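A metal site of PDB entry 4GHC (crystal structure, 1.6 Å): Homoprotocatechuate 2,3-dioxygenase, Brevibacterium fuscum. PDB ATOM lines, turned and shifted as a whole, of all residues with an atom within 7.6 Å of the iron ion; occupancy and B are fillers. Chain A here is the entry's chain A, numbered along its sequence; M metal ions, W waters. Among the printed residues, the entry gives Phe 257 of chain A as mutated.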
ATOM      1  N   ASP A 154      -6.865  25.244  11.481  1.00  0.00           N
ATOM      2  CA  ASP A 154      -7.799  26.196  10.849  1.00  0.00           C
ATOM      3  C   ASP A 154      -9.294  25.833  10.903  1.00  0.00           C
ATOM      4  O   ASP A 154     -10.102  26.689  11.217  1.00  0.00           O
ATOM      5  CB  ASP A 154      -7.435  26.503   9.387  1.00  0.00           C
ATOM      6  CG  ASP A 154      -8.231  27.690   8.852  1.00  0.00           C
ATOM      7  OD1 ASP A 154      -7.957  28.860   9.248  1.00  0.00           O
ATOM      8  OD2 ASP A 154      -9.190  27.462   8.080  1.00  0.00           O
ATOM      9  N   HIS A 155      -9.643  24.593  10.571  1.00  0.00           N
ATOM     10  CA  HIS A 155     -11.069  24.230  10.524  1.00  0.00           C
ATOM     11  C   HIS A 155     -11.324  22.758  10.474  1.00  0.00           C
ATOM     12  O   HIS A 155     -10.409  21.943  10.280  1.00  0.00           O
ATOM     13  CB  HIS A 155     -11.769  24.884   9.320  1.00  0.00           C
ATOM     14  CG  HIS A 155     -11.252  24.427   7.975  1.00  0.00           C
ATOM     15  ND1 HIS A 155     -10.284  25.089   7.293  1.00  0.00           N
ATOM     16  CD2 HIS A 155     -11.634  23.355   7.164  1.00  0.00           C
ATOM     17  CE1 HIS A 155     -10.062  24.464   6.108  1.00  0.00           C
ATOM     18  NE2 HIS A 155     -10.872  23.409   6.027  1.00  0.00           N
ATOM     19  N   PHE A 156     -12.588  22.398  10.712  1.00  0.00           N
ATOM     20  CA  PHE A 156     -13.109  21.079  10.448  1.00  0.00           C
ATOM     21  C   PHE A 156     -14.030  21.161   9.227  1.00  0.00           C
ATOM     22  O   PHE A 156     -14.474  22.242   8.837  1.00  0.00           O
ATOM     23  CB  PHE A 156     -13.970  20.616  11.637  1.00  0.00           C
ATOM     24  CG  PHE A 156     -13.305  20.774  12.994  1.00  0.00           C
ATOM     25  CD1 PHE A 156     -12.096  20.188  13.250  1.00  0.00           C
ATOM     26  CD2 PHE A 156     -13.933  21.466  14.007  1.00  0.00           C
ATOM     27  CE1 PHE A 156     -11.510  20.298  14.502  1.00  0.00           C
ATOM     28  CE2 PHE A 156     -13.369  21.583  15.266  1.00  0.00           C
ATOM     29  CZ  PHE A 156     -12.155  21.002  15.506  1.00  0.00           C
ATOM     30  N   ASN A 157     -14.302  20.011   8.618  1.00  0.00           N
ATOM     31  CA  ASN A 157     -15.321  19.921   7.568  1.00  0.00           C
ATOM     32  C   ASN A 157     -16.123  18.644   7.783  1.00  0.00           C
ATOM     33  O   ASN A 157     -15.562  17.576   7.874  1.00  0.00           O
ATOM     34  CB  ASN A 157     -14.635  19.965   6.197  1.00  0.00           C
ATOM     35  CG  ASN A 157     -15.611  20.070   5.052  1.00  0.00           C
ATOM     36  OD1 ASN A 157     -16.505  19.220   4.918  1.00  0.00           O
ATOM     37  ND2 ASN A 157     -15.440  21.096   4.195  1.00  0.00           N
ATOM     38  N   TRP A 192     -19.944  27.055   4.279  1.00  0.00           N
ATOM     39  CA  TRP A 192     -18.799  27.367   5.118  1.00  0.00           C
ATOM     40  C   TRP A 192     -19.179  28.381   6.144  1.00  0.00           C
ATOM     41  O   TRP A 192     -19.858  29.339   5.810  1.00  0.00           O
ATOM     42  CB  TRP A 192     -17.702  27.976   4.258  1.00  0.00           C
ATOM     43  CG  TRP A 192     -16.968  26.980   3.410  1.00  0.00           C
ATOM     44  CD1 TRP A 192     -15.677  26.501   3.622  1.00  0.00           C
ATOM     45  CD2 TRP A 192     -17.434  26.291   2.203  1.00  0.00           C
ATOM     46  NE1 TRP A 192     -15.313  25.589   2.648  1.00  0.00           N
ATOM     47  CE2 TRP A 192     -16.336  25.444   1.761  1.00  0.00           C
ATOM     48  CE3 TRP A 192     -18.569  26.354   1.428  1.00  0.00           C
ATOM     49  CZ2 TRP A 192     -16.415  24.657   0.625  1.00  0.00           C
ATOM     50  CZ3 TRP A 192     -18.630  25.575   0.269  1.00  0.00           C
ATOM     51  CH2 TRP A 192     -17.584  24.731  -0.108  1.00  0.00           C
ATOM     52  N   HIS A 200     -13.725  29.961   7.681  1.00  0.00           N
ATOM     53  CA  HIS A 200     -14.469  29.015   8.464  1.00  0.00           C
ATOM     54  C   HIS A 200     -13.764  28.431   9.641  1.00  0.00           C
ATOM     55  O   HIS A 200     -12.539  28.397   9.703  1.00  0.00           O
ATOM     56  CB  HIS A 200     -15.085  27.913   7.591  1.00  0.00           C
ATOM     57  CG  HIS A 200     -14.108  27.079   6.788  1.00  0.00           C
ATOM     58  ND1 HIS A 200     -13.059  27.588   6.077  1.00  0.00           N
ATOM     59  CD2 HIS A 200     -14.158  25.716   6.490  1.00  0.00           C
ATOM     60  CE1 HIS A 200     -12.487  26.588   5.384  1.00  0.00           C
ATOM     61  NE2 HIS A 200     -13.175  25.455   5.613  1.00  0.00           N
ATOM     62  N   ALA A 203     -17.494  23.482   8.386  1.00  0.00           N
ATOM     63  CA  ALA A 203     -18.163  23.514   7.107  1.00  0.00           C
ATOM     64  C   ALA A 203     -18.986  22.275   6.976  1.00  0.00           C
ATOM     65  O   ALA A 203     -18.722  21.269   7.642  1.00  0.00           O
ATOM     66  CB  ALA A 203     -17.137  23.625   5.970  1.00  0.00           C
ATOM     67  N   THR A 205     -20.497  19.649   4.148  1.00  0.00           N
ATOM     68  CA  THR A 205     -20.431  19.106   2.797  1.00  0.00           C
ATOM     69  C   THR A 205     -21.578  18.113   2.673  1.00  0.00           C
ATOM     70  O   THR A 205     -21.700  17.214   3.518  1.00  0.00           O
ATOM     71  CB  THR A 205     -19.080  18.405   2.554  1.00  0.00           C
ATOM     72  OG1 THR A 205     -18.017  19.359   2.722  1.00  0.00           O
ATOM     73  CG2 THR A 205     -19.006  17.733   1.185  1.00  0.00           C
ATOM     74  N   HIS A 213     -15.310  14.926   7.158  1.00  0.00           N
ATOM     75  CA  HIS A 213     -14.614  15.020   5.877  1.00  0.00           C
ATOM     76  C   HIS A 213     -13.129  15.242   6.059  1.00  0.00           C
ATOM     77  O   HIS A 213     -12.330  14.499   5.486  1.00  0.00           O
ATOM     78  CB  HIS A 213     -15.198  16.099   4.978  1.00  0.00           C
ATOM     79  CG  HIS A 213     -14.805  15.928   3.551  1.00  0.00           C
ATOM     80  ND1 HIS A 213     -13.586  16.294   3.089  1.00  0.00           N
ATOM     81  CD2 HIS A 213     -15.465  15.352   2.490  1.00  0.00           C
ATOM     82  CE1 HIS A 213     -13.489  15.950   1.807  1.00  0.00           C
ATOM     83  NE2 HIS A 213     -14.623  15.382   1.428  1.00  0.00           N
ATOM     84  N   HIS A 214     -12.750  16.263   6.800  1.00  0.00           N
ATOM     85  CA  HIS A 214     -11.343  16.510   7.101  1.00  0.00           C
ATOM     86  C   HIS A 214     -11.133  17.440   8.251  1.00  0.00           C
ATOM     87  O   HIS A 214     -12.058  18.101   8.740  1.00  0.00           O
ATOM     88  CB  HIS A 214     -10.600  17.032   5.852  1.00  0.00           C
ATOM     89  CG  HIS A 214     -11.158  18.311   5.259  1.00  0.00           C
ATOM     90  ND1 HIS A 214     -12.095  18.306   4.250  1.00  0.00           N
ATOM     91  CD2 HIS A 214     -10.844  19.639   5.495  1.00  0.00           C
ATOM     92  CE1 HIS A 214     -12.375  19.588   3.898  1.00  0.00           C
ATOM     93  NE2 HIS A 214     -11.611  20.411   4.658  1.00  0.00           N
ATOM     94  N   VAL A 215      -9.864  17.460   8.690  1.00  0.00           N
ATOM     95  CA  VAL A 215      -9.323  18.473   9.596  1.00  0.00           C
ATOM     96  C   VAL A 215      -8.267  19.250   8.805  1.00  0.00           C
ATOM     97  O   VAL A 215      -7.447  18.649   8.118  1.00  0.00           O
ATOM     98  CB  VAL A 215      -8.698  17.828  10.858  1.00  0.00           C
ATOM     99  CG1 VAL A 215      -8.102  18.885  11.755  1.00  0.00           C
ATOM    100  CG2 VAL A 215      -9.737  16.962  11.601  1.00  0.00           C
ATOM    101  N   ALA A 216      -8.253  20.586   8.950  1.00  0.00           N
ATOM    102  CA  ALA A 216      -7.325  21.438   8.204  1.00  0.00           C
ATOM    103  C   ALA A 216      -6.363  22.188   9.090  1.00  0.00           C
ATOM    104  O   ALA A 216      -6.776  22.814  10.077  1.00  0.00           O
ATOM    105  CB  ALA A 216      -8.100  22.416   7.312  1.00  0.00           C
ATOM    106  N   HIS A 248      -8.241  27.117  -4.038  1.00  0.00           N
ATOM    107  CA  HIS A 248      -9.693  26.962  -3.945  1.00  0.00           C
ATOM    108  C   HIS A 248     -10.360  28.166  -4.579  1.00  0.00           C
ATOM    109  O   HIS A 248      -9.824  29.280  -4.550  1.00  0.00           O
ATOM    110  CB  HIS A 248     -10.165  26.917  -2.482  1.00  0.00           C
ATOM    111  CG  HIS A 248      -9.910  25.627  -1.754  1.00  0.00           C
ATOM    112  ND1 HIS A 248     -10.337  24.408  -2.240  1.00  0.00           N
ATOM    113  CD2 HIS A 248      -9.320  25.375  -0.518  1.00  0.00           C
ATOM    114  CE1 HIS A 248     -10.035  23.445  -1.338  1.00  0.00           C
ATOM    115  NE2 HIS A 248      -9.414  24.040  -0.280  1.00  0.00           N
ATOM    116  N   SER A 251     -13.261  30.206  -0.627  1.00  0.00           N
ATOM    117  CA  SER A 251     -12.232  30.518   0.386  1.00  0.00           C
ATOM    118  C   SER A 251     -10.971  31.162  -0.152  1.00  0.00           C
ATOM    119  O   SER A 251     -10.263  31.837   0.616  1.00  0.00           O
ATOM    120  CB  SER A 251     -11.829  29.336   1.272  1.00  0.00           C
ATOM    121  OG  SER A 251     -10.840  28.518   0.660  1.00  0.00           O
ATOM    122  N   TYR A 255      -4.254  25.072  -1.133  1.00  0.00           N
ATOM    123  CA  TYR A 255      -4.624  23.851  -0.431  1.00  0.00           C
ATOM    124  C   TYR A 255      -3.968  22.571  -0.920  1.00  0.00           C
ATOM    125  O   TYR A 255      -3.428  22.510  -2.046  1.00  0.00           O
ATOM    126  CB  TYR A 255      -6.154  23.662  -0.503  1.00  0.00           C
ATOM    127  CG  TYR A 255      -6.641  23.145  -1.859  1.00  0.00           C
ATOM    128  CD1 TYR A 255      -7.013  24.025  -2.874  1.00  0.00           C
ATOM    129  CD2 TYR A 255      -6.701  21.807  -2.140  1.00  0.00           C
ATOM    130  CE1 TYR A 255      -7.450  23.572  -4.098  1.00  0.00           C
ATOM    131  CE2 TYR A 255      -7.129  21.318  -3.372  1.00  0.00           C
ATOM    132  CZ  TYR A 255      -7.495  22.208  -4.374  1.00  0.00           C
ATOM    133  OH  TYR A 255      -7.910  21.738  -5.596  1.00  0.00           O
ATOM    134  N   PHE A 257      -4.853  18.072  -0.045  1.00  0.00           N
ATOM    135  CA  PHE A 257      -5.502  17.010   0.752  1.00  0.00           C
ATOM    136  C   PHE A 257      -4.659  15.747   0.718  1.00  0.00           C
ATOM    137  O   PHE A 257      -4.282  15.266  -0.354  1.00  0.00           O
ATOM    138  CB  PHE A 257      -6.902  16.685   0.222  1.00  0.00           C
ATOM    139  CG  PHE A 257      -7.857  17.833   0.330  1.00  0.00           C
ATOM    140  CD1 PHE A 257      -8.523  18.079   1.530  1.00  0.00           C
ATOM    141  CD2 PHE A 257      -8.110  18.666  -0.750  1.00  0.00           C
ATOM    142  CE1 PHE A 257      -9.414  19.137   1.647  1.00  0.00           C
ATOM    143  CE2 PHE A 257      -9.013  19.732  -0.634  1.00  0.00           C
ATOM    144  CZ  PHE A 257      -9.639  19.971   0.560  1.00  0.00           C
ATOM    145  N   GLU A 267      -6.299  18.348   5.460  1.00  0.00           N
ATOM    146  CA  GLU A 267      -6.077  19.443   4.503  1.00  0.00           C
ATOM    147  C   GLU A 267      -4.983  20.344   5.056  1.00  0.00           C
ATOM    148  O   GLU A 267      -4.935  20.615   6.256  1.00  0.00           O
ATOM    149  CB  GLU A 267      -7.349  20.272   4.274  1.00  0.00           C
ATOM    150  CG  GLU A 267      -7.188  21.312   3.185  1.00  0.00           C
ATOM    151  CD  GLU A 267      -8.455  22.144   2.991  1.00  0.00           C
ATOM    152  OE1 GLU A 267      -9.379  22.015   3.813  1.00  0.00           O
ATOM    153  OE2 GLU A 267      -8.519  22.962   2.027  1.00  0.00           O
ATOM    154  N   ILE A 268      -4.122  20.812   4.154  1.00  0.00           N
ATOM    155  CA  ILE A 268      -3.172  21.876   4.462  1.00  0.00           C
ATOM    156  C   ILE A 268      -3.671  23.092   3.672  1.00  0.00           C
ATOM    157  O   ILE A 268      -4.056  22.962   2.499  1.00  0.00           O
ATOM    158  CB  ILE A 268      -1.717  21.507   4.081  1.00  0.00           C
ATOM    159  CG1 ILE A 268      -1.436  19.998   4.354  1.00  0.00           C
ATOM    160  CG2 ILE A 268      -0.779  22.487   4.765  1.00  0.00           C
ATOM    161  CD1 ILE A 268      -1.479  19.633   5.808  1.00  0.00           C
ATOM    162  N   TYR A 269      -3.652  24.260   4.303  1.00  0.00           N
ATOM    163  CA  TYR A 269      -4.427  25.407   3.854  1.00  0.00           C
ATOM    164  C   TYR A 269      -3.704  26.709   4.147  1.00  0.00           C
ATOM    165  O   TYR A 269      -3.060  26.823   5.204  1.00  0.00           O
ATOM    166  CB  TYR A 269      -5.730  25.323   4.644  1.00  0.00           C
ATOM    167  CG  TYR A 269      -6.839  26.332   4.471  1.00  0.00           C
ATOM    168  CD1 TYR A 269      -7.923  26.062   3.631  1.00  0.00           C
ATOM    169  CD2 TYR A 269      -6.873  27.490   5.227  1.00  0.00           C
ATOM    170  CE1 TYR A 269      -9.018  26.945   3.554  1.00  0.00           C
ATOM    171  CE2 TYR A 269      -7.927  28.376   5.135  1.00  0.00           C
ATOM    172  CZ  TYR A 269      -9.007  28.090   4.298  1.00  0.00           C
ATOM    173  OH  TYR A 269     -10.100  28.917   4.210  1.00  0.00           O
ATOM    174  N   ARG A 293     -14.133  24.824  -6.720  1.00  0.00           N
ATOM    175  CA  ARG A 293     -13.404  24.007  -5.744  1.00  0.00           C
ATOM    176  C   ARG A 293     -11.900  24.072  -6.000  1.00  0.00           C
ATOM    177  O   ARG A 293     -11.114  24.227  -5.068  1.00  0.00           O
ATOM    178  CB  ARG A 293     -13.905  22.569  -5.733  1.00  0.00           C
ATOM    179  CG  ARG A 293     -15.252  22.438  -5.034  1.00  0.00           C
ATOM    180  CD  ARG A 293     -15.543  21.018  -4.597  1.00  0.00           C
ATOM    181  NE  ARG A 293     -16.811  20.934  -3.857  1.00  0.00           N
ATOM    182  CZ  ARG A 293     -16.948  21.208  -2.562  1.00  0.00           C
ATOM    183  NH1 ARG A 293     -15.923  21.619  -1.791  1.00  0.00           N
ATOM    184  NH2 ARG A 293     -18.122  21.053  -1.983  1.00  0.00           N
ATOM    185  N   TRP A 304     -12.771  12.274  -3.059  1.00  0.00           N
ATOM    186  CA  TRP A 304     -13.052  13.449  -2.260  1.00  0.00           C
ATOM    187  C   TRP A 304     -14.509  13.550  -1.972  1.00  0.00           C
ATOM    188  O   TRP A 304     -14.916  14.025  -0.920  1.00  0.00           O
ATOM    189  CB  TRP A 304     -12.501  14.698  -2.992  1.00  0.00           C
ATOM    190  CG  TRP A 304     -12.285  15.866  -2.075  1.00  0.00           C
ATOM    191  CD1 TRP A 304     -11.123  16.175  -1.366  1.00  0.00           C
ATOM    192  CD2 TRP A 304     -13.269  16.849  -1.661  1.00  0.00           C
ATOM    193  NE1 TRP A 304     -11.333  17.290  -0.577  1.00  0.00           N
ATOM    194  CE2 TRP A 304     -12.586  17.751  -0.721  1.00  0.00           C
ATOM    195  CE3 TRP A 304     -14.602  17.069  -1.959  1.00  0.00           C
ATOM    196  CZ2 TRP A 304     -13.241  18.792  -0.107  1.00  0.00           C
ATOM    197  CZ3 TRP A 304     -15.256  18.134  -1.350  1.00  0.00           C
ATOM    198  CH2 TRP A 304     -14.600  18.976  -0.426  1.00  0.00           C
HETATM  199 FE    FE M   1     -11.348  22.487   4.087  1.00  0.00          FE
HETATM  200  O   HOH W   1     -10.886  24.344   3.066  1.00  0.00           O
HETATM  201  O   HOH W   2     -12.049  21.904   1.991  1.00  0.00           O
HETATM  202  O   HOH W   3     -13.382  23.102   4.284  1.00  0.00           O
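The iron ion is bound by OE1 of Glu 267, water W3, NE2 of His 214, water W1, NE2 of His 155 and water W2.
The iron ion has six donor atoms within binding distance.
Residues that only touch the iron ion: His 200 (3.8 Å).
Of the 21 residues printed, 4 come within 4 Å of the iron ion.
Along chain A the residues within 4 Å of the iron ion span positions 155 to 267.
The nearest printed residue that does not touch the iron ion is Asn 157 (4.3 Å).
Water W3 lies within hydrogen-bond range of a ring nitrogen (NE2) of His 200 (2.7 Å) and the side-chain amide nitrogen (ND2) of Asn 157 (2.9 Å).
NE2 of His 248 lies within hydrogen-bond range of OE2 of Glu 267, 2.7 Å away.
The backbone NH of Glu 267 lies within hydrogen-bond range of the backbone carbonyl oxygen of Val 215 (2.9 Å).
N of Asn 157 is in hydrogen-bond range of O of His 214 (2.9 Å).
ND1 of His 214 lies within hydrogen-bond range of ND1 of His 213 (2.8 Å).
A ring nitrogen (NE2) of His 200 lies close to a ring nitrogen (ND1) of His 155 (3.4 Å).
The backbone carbonyl oxygen of His 155 sits at hydrogen-bond distance from the backbone NH of Ala 216 (2.9 Å).
ND1 of His 155 sits at hydrogen-bond distance from OD2 of Asp 154 (2.7 Å).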
